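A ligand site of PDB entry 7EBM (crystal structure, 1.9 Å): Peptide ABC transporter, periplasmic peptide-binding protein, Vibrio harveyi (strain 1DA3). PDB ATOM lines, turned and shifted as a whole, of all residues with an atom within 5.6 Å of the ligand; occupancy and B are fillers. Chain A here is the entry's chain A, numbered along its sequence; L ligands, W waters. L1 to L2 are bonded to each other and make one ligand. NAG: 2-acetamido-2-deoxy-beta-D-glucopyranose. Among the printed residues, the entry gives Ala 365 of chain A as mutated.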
ATOM      1  N   HIS A   9     -10.882 -17.632 -16.548  1.00  0.00           N
ATOM      2  CA  HIS A   9     -12.136 -16.916 -16.848  1.00  0.00           C
ATOM      3  C   HIS A   9     -11.876 -15.827 -17.913  1.00  0.00           C
ATOM      4  O   HIS A   9     -11.603 -14.683 -17.589  1.00  0.00           O
ATOM      5  CB  HIS A   9     -12.703 -16.295 -15.570  1.00  0.00           C
ATOM      6  CG  HIS A   9     -13.939 -15.478 -15.781  1.00  0.00           C
ATOM      7  ND1 HIS A   9     -14.987 -15.885 -16.593  1.00  0.00           N
ATOM      8  CD2 HIS A   9     -14.303 -14.282 -15.277  1.00  0.00           C
ATOM      9  CE1 HIS A   9     -15.927 -14.961 -16.584  1.00  0.00           C
ATOM     10  NE2 HIS A   9     -15.548 -13.975 -15.788  1.00  0.00           N
ATOM     11  N   PRO A  10     -11.917 -16.195 -19.201  1.00  0.00           N
ATOM     12  CA  PRO A  10     -11.570 -15.198 -20.224  1.00  0.00           C
ATOM     13  C   PRO A  10     -12.730 -14.274 -20.602  1.00  0.00           C
ATOM     14  O   PRO A  10     -12.481 -13.167 -21.088  1.00  0.00           O
ATOM     15  CB  PRO A  10     -11.149 -16.058 -21.418  1.00  0.00           C
ATOM     16  CG  PRO A  10     -11.937 -17.374 -21.219  1.00  0.00           C
ATOM     17  CD  PRO A  10     -11.931 -17.579 -19.730  1.00  0.00           C
ATOM     18  N   LYS A  11     -13.974 -14.689 -20.365  1.00  0.00           N
ATOM     19  CA  LYS A  11     -15.118 -14.005 -20.958  1.00  0.00           C
ATOM     20  C   LYS A  11     -16.421 -14.324 -20.221  1.00  0.00           C
ATOM     21  O   LYS A  11     -16.699 -15.481 -19.883  1.00  0.00           O
ATOM     22  CB  LYS A  11     -15.234 -14.394 -22.442  1.00  0.00           C
ATOM     23  CG  LYS A  11     -16.473 -13.868 -23.178  1.00  0.00           C
ATOM     24  CD  LYS A  11     -16.389 -12.390 -23.428  1.00  0.00           C
ATOM     25  CE  LYS A  11     -17.542 -11.956 -24.312  1.00  0.00           C
ATOM     26  NZ  LYS A  11     -17.775 -10.495 -24.175  1.00  0.00           N
ATOM     27  N   GLU A  12     -17.237 -13.301 -19.983  1.00  0.00           N
ATOM     28  CA  GLU A  12     -18.548 -13.510 -19.359  1.00  0.00           C
ATOM     29  C   GLU A  12     -19.498 -14.197 -20.297  1.00  0.00           C
ATOM     30  O   GLU A  12     -19.570 -13.866 -21.462  1.00  0.00           O
ATOM     31  CB  GLU A  12     -19.144 -12.198 -18.915  1.00  0.00           C
ATOM     32  CG  GLU A  12     -18.202 -11.391 -18.060  1.00  0.00           C
ATOM     33  CD  GLU A  12     -17.378 -10.365 -18.859  1.00  0.00           C
ATOM     34  OE1 GLU A  12     -17.083 -10.592 -20.073  1.00  0.00           O
ATOM     35  OE2 GLU A  12     -17.016  -9.343 -18.261  1.00  0.00           O
ATOM     36  N   HIS A  30     -14.118 -18.277 -25.747  1.00  0.00           N
ATOM     37  CA  HIS A  30     -12.895 -17.491 -25.779  1.00  0.00           C
ATOM     38  C   HIS A  30     -11.642 -18.222 -25.345  1.00  0.00           C
ATOM     39  O   HIS A  30     -10.695 -17.599 -24.852  1.00  0.00           O
ATOM     40  CB  HIS A  30     -13.071 -16.239 -24.943  1.00  0.00           C
ATOM     41  CG  HIS A  30     -13.901 -15.204 -25.614  1.00  0.00           C
ATOM     42  ND1 HIS A  30     -13.640 -13.857 -25.515  1.00  0.00           N
ATOM     43  CD2 HIS A  30     -14.960 -15.322 -26.445  1.00  0.00           C
ATOM     44  CE1 HIS A  30     -14.526 -13.186 -26.232  1.00  0.00           C
ATOM     45  NE2 HIS A  30     -15.350 -14.051 -26.800  1.00  0.00           N
ATOM     46  N   ASN A 206     -19.440  -9.325 -12.888  1.00  0.00           N
ATOM     47  CA  ASN A 206     -18.389  -9.127 -11.886  1.00  0.00           C
ATOM     48  C   ASN A 206     -18.854  -9.525 -10.500  1.00  0.00           C
ATOM     49  O   ASN A 206     -18.018  -9.873  -9.648  1.00  0.00           O
ATOM     50  CB  ASN A 206     -17.897  -7.674 -11.861  1.00  0.00           C
ATOM     51  CG  ASN A 206     -16.948  -7.353 -13.021  1.00  0.00           C
ATOM     52  OD1 ASN A 206     -16.536  -8.242 -13.769  1.00  0.00           O
ATOM     53  ND2 ASN A 206     -16.631  -6.072 -13.180  1.00  0.00           N
ATOM     54  N   SER A 222      -8.692 -12.099 -15.090  1.00  0.00           N
ATOM     55  CA  SER A 222      -8.361 -10.735 -15.470  1.00  0.00           C
ATOM     56  C   SER A 222      -9.577  -9.827 -15.299  1.00  0.00           C
ATOM     57  O   SER A 222      -9.792  -8.914 -16.090  1.00  0.00           O
ATOM     58  CB  SER A 222      -7.851 -10.707 -16.923  1.00  0.00           C
ATOM     59  OG  SER A 222      -6.586 -11.357 -17.020  1.00  0.00           O
ATOM     60  N   SER A 223     -10.393 -10.106 -14.278  1.00  0.00           N
ATOM     61  CA  SER A 223     -11.607  -9.328 -14.043  1.00  0.00           C
ATOM     62  C   SER A 223     -11.366  -8.164 -13.118  1.00  0.00           C
ATOM     63  O   SER A 223     -10.420  -8.158 -12.312  1.00  0.00           O
ATOM     64  CB  SER A 223     -12.703 -10.212 -13.442  1.00  0.00           C
ATOM     65  OG  SER A 223     -13.246 -11.093 -14.398  1.00  0.00           O
ATOM     66  N   PHE A 224     -12.226  -7.152 -13.202  1.00  0.00           N
ATOM     67  CA  PHE A 224     -12.201  -6.097 -12.212  1.00  0.00           C
ATOM     68  C   PHE A 224     -12.648  -6.665 -10.873  1.00  0.00           C
ATOM     69  O   PHE A 224     -13.633  -7.391 -10.776  1.00  0.00           O
ATOM     70  CB  PHE A 224     -13.094  -4.906 -12.613  1.00  0.00           C
ATOM     71  CG  PHE A 224     -13.300  -3.914 -11.492  1.00  0.00           C
ATOM     72  CD1 PHE A 224     -12.287  -3.044 -11.131  1.00  0.00           C
ATOM     73  CD2 PHE A 224     -14.502  -3.869 -10.797  1.00  0.00           C
ATOM     74  CE1 PHE A 224     -12.465  -2.128 -10.100  1.00  0.00           C
ATOM     75  CE2 PHE A 224     -14.686  -2.963  -9.786  1.00  0.00           C
ATOM     76  CZ  PHE A 224     -13.669  -2.086  -9.430  1.00  0.00           C
ATOM     77  N   GLN A 249      -9.077   4.443 -22.255  1.00  0.00           N
ATOM     78  CA  GLN A 249     -10.535   4.288 -22.124  1.00  0.00           C
ATOM     79  C   GLN A 249     -11.172   5.640 -22.372  1.00  0.00           C
ATOM     80  O   GLN A 249     -10.655   6.667 -21.918  1.00  0.00           O
ATOM     81  CB  GLN A 249     -10.920   3.748 -20.746  1.00  0.00           C
ATOM     82  CG  GLN A 249     -10.286   2.396 -20.444  1.00  0.00           C
ATOM     83  CD  GLN A 249     -10.711   1.795 -19.126  1.00  0.00           C
ATOM     84  OE1 GLN A 249     -11.603   2.308 -18.438  1.00  0.00           O
ATOM     85  NE2 GLN A 249     -10.064   0.697 -18.752  1.00  0.00           N
ATOM     86  N   PHE A 289     -12.618   2.630 -10.096  1.00  0.00           N
ATOM     87  CA  PHE A 289     -11.544   1.661 -10.315  1.00  0.00           C
ATOM     88  C   PHE A 289     -10.651   1.483  -9.093  1.00  0.00           C
ATOM     89  O   PHE A 289      -9.585   0.870  -9.188  1.00  0.00           O
ATOM     90  CB  PHE A 289     -10.679   2.070 -11.501  1.00  0.00           C
ATOM     91  CG  PHE A 289     -11.398   2.083 -12.817  1.00  0.00           C
ATOM     92  CD1 PHE A 289     -11.392   0.956 -13.643  1.00  0.00           C
ATOM     93  CD2 PHE A 289     -12.041   3.228 -13.260  1.00  0.00           C
ATOM     94  CE1 PHE A 289     -12.049   0.976 -14.889  1.00  0.00           C
ATOM     95  CE2 PHE A 289     -12.686   3.258 -14.500  1.00  0.00           C
ATOM     96  CZ  PHE A 289     -12.700   2.127 -15.311  1.00  0.00           C
ATOM     97  N   GLY A 364     -22.459  -6.077 -16.549  1.00  0.00           N
ATOM     98  CA  GLY A 364     -21.557  -6.872 -15.745  1.00  0.00           C
ATOM     99  C   GLY A 364     -20.201  -6.210 -15.522  1.00  0.00           C
ATOM    100  O   GLY A 364     -19.447  -6.630 -14.632  1.00  0.00           O
ATOM    101  N   ALA A 365     -19.885  -5.207 -16.338  1.00  0.00           N
ATOM    102  CA  ALA A 365     -18.615  -4.507 -16.244  1.00  0.00           C
ATOM    103  C   ALA A 365     -18.771  -3.375 -15.257  1.00  0.00           C
ATOM    104  O   ALA A 365     -18.822  -2.209 -15.640  1.00  0.00           O
ATOM    105  CB  ALA A 365     -18.151  -3.986 -17.607  1.00  0.00           C
ATOM    106  N   THR A 366     -18.851  -3.738 -13.978  1.00  0.00           N
ATOM    107  CA  THR A 366     -19.235  -2.785 -12.932  1.00  0.00           C
ATOM    108  C   THR A 366     -18.298  -1.573 -12.796  1.00  0.00           C
ATOM    109  O   THR A 366     -18.745  -0.475 -12.460  1.00  0.00           O
ATOM    110  CB  THR A 366     -19.361  -3.512 -11.575  1.00  0.00           C
ATOM    111  OG1 THR A 366     -18.172  -4.276 -11.324  1.00  0.00           O
ATOM    112  CG2 THR A 366     -20.513  -4.480 -11.612  1.00  0.00           C
ATOM    113  N   ASP A 367     -17.000  -1.750 -13.073  1.00  0.00           N
ATOM    114  CA  ASP A 367     -16.083  -0.611 -13.050  1.00  0.00           C
ATOM    115  C   ASP A 367     -16.451   0.410 -14.138  1.00  0.00           C
ATOM    116  O   ASP A 367     -16.457   1.620 -13.890  1.00  0.00           O
ATOM    117  CB  ASP A 367     -14.619  -1.082 -13.197  1.00  0.00           C
ATOM    118  CG  ASP A 367     -14.394  -2.007 -14.402  1.00  0.00           C
ATOM    119  OD1 ASP A 367     -15.350  -2.694 -14.853  1.00  0.00           O
ATOM    120  OD2 ASP A 367     -13.238  -2.063 -14.892  1.00  0.00           O
ATOM    121  N   PHE A 368     -16.770  -0.076 -15.336  1.00  0.00           N
ATOM    122  CA  PHE A 368     -17.231   0.804 -16.393  1.00  0.00           C
ATOM    123  C   PHE A 368     -18.625   1.340 -16.076  1.00  0.00           C
ATOM    124  O   PHE A 368     -18.917   2.499 -16.382  1.00  0.00           O
ATOM    125  CB  PHE A 368     -17.276   0.065 -17.740  1.00  0.00           C
ATOM    126  CG  PHE A 368     -15.916  -0.198 -18.349  1.00  0.00           C
ATOM    127  CD1 PHE A 368     -14.753  -0.005 -17.624  1.00  0.00           C
ATOM    128  CD2 PHE A 368     -15.816  -0.641 -19.670  1.00  0.00           C
ATOM    129  CE1 PHE A 368     -13.500  -0.260 -18.176  1.00  0.00           C
ATOM    130  CE2 PHE A 368     -14.575  -0.883 -20.236  1.00  0.00           C
ATOM    131  CZ  PHE A 368     -13.411  -0.687 -19.486  1.00  0.00           C
ATOM    132  N   ASN A 411     -13.073   0.617 -23.596  1.00  0.00           N
ATOM    133  CA  ASN A 411     -11.624   0.565 -23.677  1.00  0.00           C
ATOM    134  C   ASN A 411     -11.180   0.133 -25.063  1.00  0.00           C
ATOM    135  O   ASN A 411     -11.992  -0.139 -25.961  1.00  0.00           O
ATOM    136  CB  ASN A 411     -11.038  -0.369 -22.606  1.00  0.00           C
ATOM    137  CG  ASN A 411     -11.588  -1.753 -22.676  1.00  0.00           C
ATOM    138  OD1 ASN A 411     -12.616  -1.987 -23.302  1.00  0.00           O
ATOM    139  ND2 ASN A 411     -10.925  -2.684 -22.017  1.00  0.00           N
ATOM    140  N   TYR A 412      -9.864   0.120 -25.227  1.00  0.00           N
ATOM    141  CA  TYR A 412      -9.233  -0.180 -26.486  1.00  0.00           C
ATOM    142  C   TYR A 412      -8.100  -1.122 -26.232  1.00  0.00           C
ATOM    143  O   TYR A 412      -7.504  -1.097 -25.159  1.00  0.00           O
ATOM    144  CB  TYR A 412      -8.673   1.066 -27.132  1.00  0.00           C
ATOM    145  CG  TYR A 412      -9.685   2.113 -27.475  1.00  0.00           C
ATOM    146  CD1 TYR A 412     -10.261   2.154 -28.727  1.00  0.00           C
ATOM    147  CD2 TYR A 412     -10.024   3.080 -26.556  1.00  0.00           C
ATOM    148  CE1 TYR A 412     -11.180   3.126 -29.056  1.00  0.00           C
ATOM    149  CE2 TYR A 412     -10.937   4.061 -26.865  1.00  0.00           C
ATOM    150  CZ  TYR A 412     -11.512   4.072 -28.118  1.00  0.00           C
ATOM    151  OH  TYR A 412     -12.405   5.057 -28.441  1.00  0.00           O
ATOM    152  N   PHE A 413      -7.750  -1.905 -27.247  1.00  0.00           N
ATOM    153  CA  PHE A 413      -6.510  -2.659 -27.160  1.00  0.00           C
ATOM    154  C   PHE A 413      -5.323  -1.701 -27.178  1.00  0.00           C
ATOM    155  O   PHE A 413      -5.414  -0.586 -27.684  1.00  0.00           O
ATOM    156  CB  PHE A 413      -6.444  -3.683 -28.287  1.00  0.00           C
ATOM    157  CG  PHE A 413      -7.308  -4.887 -28.039  1.00  0.00           C
ATOM    158  CD1 PHE A 413      -6.906  -5.878 -27.162  1.00  0.00           C
ATOM    159  CD2 PHE A 413      -8.538  -5.017 -28.655  1.00  0.00           C
ATOM    160  CE1 PHE A 413      -7.716  -6.985 -26.926  1.00  0.00           C
ATOM    161  CE2 PHE A 413      -9.343  -6.118 -28.423  1.00  0.00           C
ATOM    162  CZ  PHE A 413      -8.935  -7.101 -27.552  1.00  0.00           C
ATOM    163  N   ARG A 438     -15.926  -2.803 -32.413  1.00  0.00           N
ATOM    164  CA  ARG A 438     -16.670  -1.565 -32.154  1.00  0.00           C
ATOM    165  C   ARG A 438     -15.814  -0.294 -32.193  1.00  0.00           C
ATOM    166  O   ARG A 438     -16.345   0.812 -32.271  1.00  0.00           O
ATOM    167  CB  ARG A 438     -17.322  -1.666 -30.781  1.00  0.00           C
ATOM    168  CG  ARG A 438     -16.286  -1.641 -29.692  1.00  0.00           C
ATOM    169  CD  ARG A 438     -16.873  -2.164 -28.416  1.00  0.00           C
ATOM    170  NE  ARG A 438     -15.915  -2.171 -27.311  1.00  0.00           N
ATOM    171  CZ  ARG A 438     -15.107  -3.183 -27.031  1.00  0.00           C
ATOM    172  NH1 ARG A 438     -15.083  -4.274 -27.791  1.00  0.00           N
ATOM    173  NH2 ARG A 438     -14.286  -3.102 -25.987  1.00  0.00           N
ATOM    174  N   PHE A 439     -14.490  -0.471 -32.140  1.00  0.00           N
ATOM    175  CA  PHE A 439     -13.581   0.592 -31.711  1.00  0.00           C
ATOM    176  C   PHE A 439     -13.597   1.851 -32.566  1.00  0.00           C
ATOM    177  O   PHE A 439     -13.393   2.954 -32.039  1.00  0.00           O
ATOM    178  CB  PHE A 439     -12.167   0.040 -31.630  1.00  0.00           C
ATOM    179  CG  PHE A 439     -12.057  -1.148 -30.744  1.00  0.00           C
ATOM    180  CD1 PHE A 439     -12.274  -1.029 -29.365  1.00  0.00           C
ATOM    181  CD2 PHE A 439     -11.767  -2.401 -31.262  1.00  0.00           C
ATOM    182  CE1 PHE A 439     -12.203  -2.137 -28.529  1.00  0.00           C
ATOM    183  CE2 PHE A 439     -11.686  -3.496 -30.436  1.00  0.00           C
ATOM    184  CZ  PHE A 439     -11.908  -3.361 -29.060  1.00  0.00           C
ATOM    185  N   MET A 491      -5.838  -5.792 -15.651  1.00  0.00           N
ATOM    186  CA  MET A 491      -6.206  -6.466 -14.408  1.00  0.00           C
ATOM    187  C   MET A 491      -5.822  -7.914 -14.532  1.00  0.00           C
ATOM    188  O   MET A 491      -6.086  -8.562 -15.561  1.00  0.00           O
ATOM    189  CB  MET A 491      -7.699  -6.371 -14.087  1.00  0.00           C
ATOM    190  CG  MET A 491      -8.291  -4.982 -14.091  1.00  0.00           C
ATOM    191  SD  MET A 491      -9.061  -4.627 -15.685  1.00  0.00           S
ATOM    192  CE  MET A 491     -10.513  -5.669 -15.674  1.00  0.00           C
ATOM    193  N   TRP A 515      -7.534 -12.841 -21.362  1.00  0.00           N
ATOM    194  CA  TRP A 515      -8.483 -12.514 -22.429  1.00  0.00           C
ATOM    195  C   TRP A 515      -8.112 -13.031 -23.804  1.00  0.00           C
ATOM    196  O   TRP A 515      -6.933 -13.079 -24.146  1.00  0.00           O
ATOM    197  CB  TRP A 515      -8.620 -10.996 -22.560  1.00  0.00           C
ATOM    198  CG  TRP A 515      -9.046 -10.307 -21.322  1.00  0.00           C
ATOM    199  CD1 TRP A 515      -9.908 -10.770 -20.373  1.00  0.00           C
ATOM    200  CD2 TRP A 515      -8.610  -9.020 -20.884  1.00  0.00           C
ATOM    201  NE1 TRP A 515     -10.042  -9.834 -19.367  1.00  0.00           N
ATOM    202  CE2 TRP A 515      -9.259  -8.754 -19.665  1.00  0.00           C
ATOM    203  CE3 TRP A 515      -7.741  -8.063 -21.424  1.00  0.00           C
ATOM    204  CZ2 TRP A 515      -9.058  -7.557 -18.965  1.00  0.00           C
ATOM    205  CZ3 TRP A 515      -7.550  -6.886 -20.721  1.00  0.00           C
ATOM    206  CH2 TRP A 515      -8.201  -6.640 -19.512  1.00  0.00           C
ATOM    207  N   ALA A 516      -9.117 -13.378 -24.609  1.00  0.00           N
ATOM    208  CA  ALA A 516      -8.884 -13.546 -26.035  1.00  0.00           C
ATOM    209  C   ALA A 516      -8.342 -12.233 -26.595  1.00  0.00           C
ATOM    210  O   ALA A 516      -8.724 -11.151 -26.140  1.00  0.00           O
ATOM    211  CB  ALA A 516     -10.177 -13.970 -26.748  1.00  0.00           C
HETATM  212  C1  NAG L   1     -11.864  -7.955 -23.749  1.00  0.00           C
HETATM  213  C2  NAG L   1     -12.042  -6.530 -23.205  1.00  0.00           C
HETATM  214  C3  NAG L   1     -11.938  -6.597 -21.690  1.00  0.00           C
HETATM  215  C4  NAG L   1     -12.939  -7.596 -21.106  1.00  0.00           C
HETATM  216  C5  NAG L   1     -12.876  -8.923 -21.865  1.00  0.00           C
HETATM  217  C6  NAG L   1     -13.939  -9.926 -21.421  1.00  0.00           C
HETATM  218  C7  NAG L   1     -11.301  -4.886 -24.834  1.00  0.00           C
HETATM  219  C8  NAG L   1     -10.191  -3.995 -25.317  1.00  0.00           C
HETATM  220  N2  NAG L   1     -11.073  -5.585 -23.719  1.00  0.00           N
HETATM  221  O1  NAG L   1     -11.872  -7.983 -25.176  1.00  0.00           O
HETATM  222  O3  NAG L   1     -12.186  -5.280 -21.183  1.00  0.00           O
HETATM  223  O4  NAG L   1     -12.646  -7.811 -19.727  1.00  0.00           O
HETATM  224  O5  NAG L   1     -12.970  -8.726 -23.278  1.00  0.00           O
HETATM  225  O6  NAG L   1     -15.245  -9.340 -21.503  1.00  0.00           O
HETATM  226  O7  NAG L   1     -12.360  -4.963 -25.444  1.00  0.00           O
HETATM  227  C1  NAG L   2     -13.638  -7.233 -18.884  1.00  0.00           C
HETATM  228  C2  NAG L   2     -13.656  -7.988 -17.553  1.00  0.00           C
HETATM  229  C3  NAG L   2     -14.585  -7.296 -16.559  1.00  0.00           C
HETATM  230  C4  NAG L   2     -14.272  -5.802 -16.449  1.00  0.00           C
HETATM  231  C5  NAG L   2     -14.285  -5.203 -17.861  1.00  0.00           C
HETATM  232  C6  NAG L   2     -13.971  -3.716 -17.853  1.00  0.00           C
HETATM  233  C7  NAG L   2     -13.324 -10.415 -17.724  1.00  0.00           C
HETATM  234  C8  NAG L   2     -13.966 -11.737 -18.013  1.00  0.00           C
HETATM  235  N2  NAG L   2     -14.133  -9.348 -17.727  1.00  0.00           N
HETATM  236  O3  NAG L   2     -14.465  -7.950 -15.285  1.00  0.00           O
HETATM  237  O4  NAG L   2     -15.239  -5.153 -15.625  1.00  0.00           O
HETATM  238  O5  NAG L   2     -13.296  -5.871 -18.650  1.00  0.00           O
HETATM  239  O6  NAG L   2     -12.791  -3.383 -17.103  1.00  0.00           O
HETATM  240  O7  NAG L   2     -12.133 -10.309 -17.499  1.00  0.00           O
HETATM  241  O   HOH W   1     -14.862  -4.008 -22.136  1.00  0.00           O
HETATM  242  O   HOH W   2     -13.661  -6.688 -27.085  1.00  0.00           O
HETATM  243  O   HOH W   3     -10.364  -2.149 -17.692  1.00  0.00           O
HETATM  244  O   HOH W   4     -11.290 -10.563 -25.563  1.00  0.00           O
HETATM  245  O   HOH W   5     -15.481  -9.287 -25.061  1.00  0.00           O
HETATM  246  O   HOH W   6     -11.353 -12.641 -15.990  1.00  0.00           O
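An oxygen (O4) of NAG L2 sits at hydrogen-bond distance from the side-chain carboxylate (OD1) of Asp 367 (2.6 Å). An oxygen (O3) of NAG L2 is in hydrogen-bond range of the side-chain amide oxygen (OD1) of Asn 206 (2.6 Å). OE1 of Glu 12 lies within hydrogen-bond range of O6 of NAG L1, at 2.6 Å. O7 of NAG L1 is in hydrogen-bond range of NH2 of Arg 438, at 2.7 Å. The indole nitrogen (NE1) of Trp 515 sits at hydrogen-bond distance from an oxygen (O7) of NAG L2, at 2.8 Å. O3 of NAG L1 sits at hydrogen-bond distance from ND2 of Asn 411 (3.0 Å). N of Phe 224 lies within hydrogen-bond range of O3 of NAG L2 (3.2 Å). OG of Ser 223 is in hydrogen-bond range of O7 of NAG L2, 3.4 Å away.
Water W4 lies within hydrogen-bond range of O1 of NAG L1 and O of Ala 516. Water W2 bridges O7 of NAG L1 (2.7 Å) and NH1 of Arg 438 (2.9 Å). Water W3 lies within hydrogen-bond range of an oxygen (O6) of NAG L2 (2.8 Å), the side-chain amide nitrogen of Gln 249 (3.1 Å) and the side-chain sulfur of Met 491 (3.4 Å). Water W6 lies within hydrogen-bond range of the backbone carbonyl oxygen (O) of His 9 (2.6 Å), the backbone NH (N) of Ser 222 (2.9 Å), an oxygen (O7) of NAG L2 (2.9 Å) and the side-chain hydroxyl (OG) of Ser 223 (2.9 Å). Water W1 bridges an oxygen (O3) of NAG L1 (3.1 Å) and the side-chain amide oxygen of Asn 411 (3.2 Å). Water W5 lies within hydrogen-bond range of the side-chain amino group (NZ) of Lys 11 and an oxygen (O5) of NAG L1.
ND2 of Asn 206 lies within hydrogen-bond range of OG1 of Thr 366 (3.0 Å). The backbone NH (N) of Asn 206 lies close to the backbone carbonyl oxygen (O) of Gly 364, at 3.2 Å. NH2 of Arg 438 sits at hydrogen-bond distance from OD1 of Asn 411 (3.4 Å). The indole nitrogen (NE1) of Trp 515 lies close to the backbone carbonyl oxygen (O) of Ser 222 (3.4 Å). O of Met 491 lies close to OG of Ser 222 (3.2 Å).
The backbone carbonyl oxygen (O) of Ser 222 lies close to an oxygen (O7) of NAG L2 (3.1 Å). Merely in contact with the ligand: Phe 368, Ala 365, Met 491, His 9, Pro 10, Tyr 412, Phe 413, Lys 11 and Phe 439. Hydrophobic or aromatic side chains that line the ligand: His 9, Phe 224, Ala 365, Phe 368, Phe 413, Phe 439, Met 491 and Trp 515. 18 residues have an atom within 4 Å of the ligand: His 9, Pro 10, Lys 11, Glu 12, Asn 206, Ser 222, Ser 223, Phe 224, Ala 365, Asp 367, Phe 368, Asn 411, Tyr 412, Phe 413, Arg 438, Phe 439, Met 491 and Trp 515.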
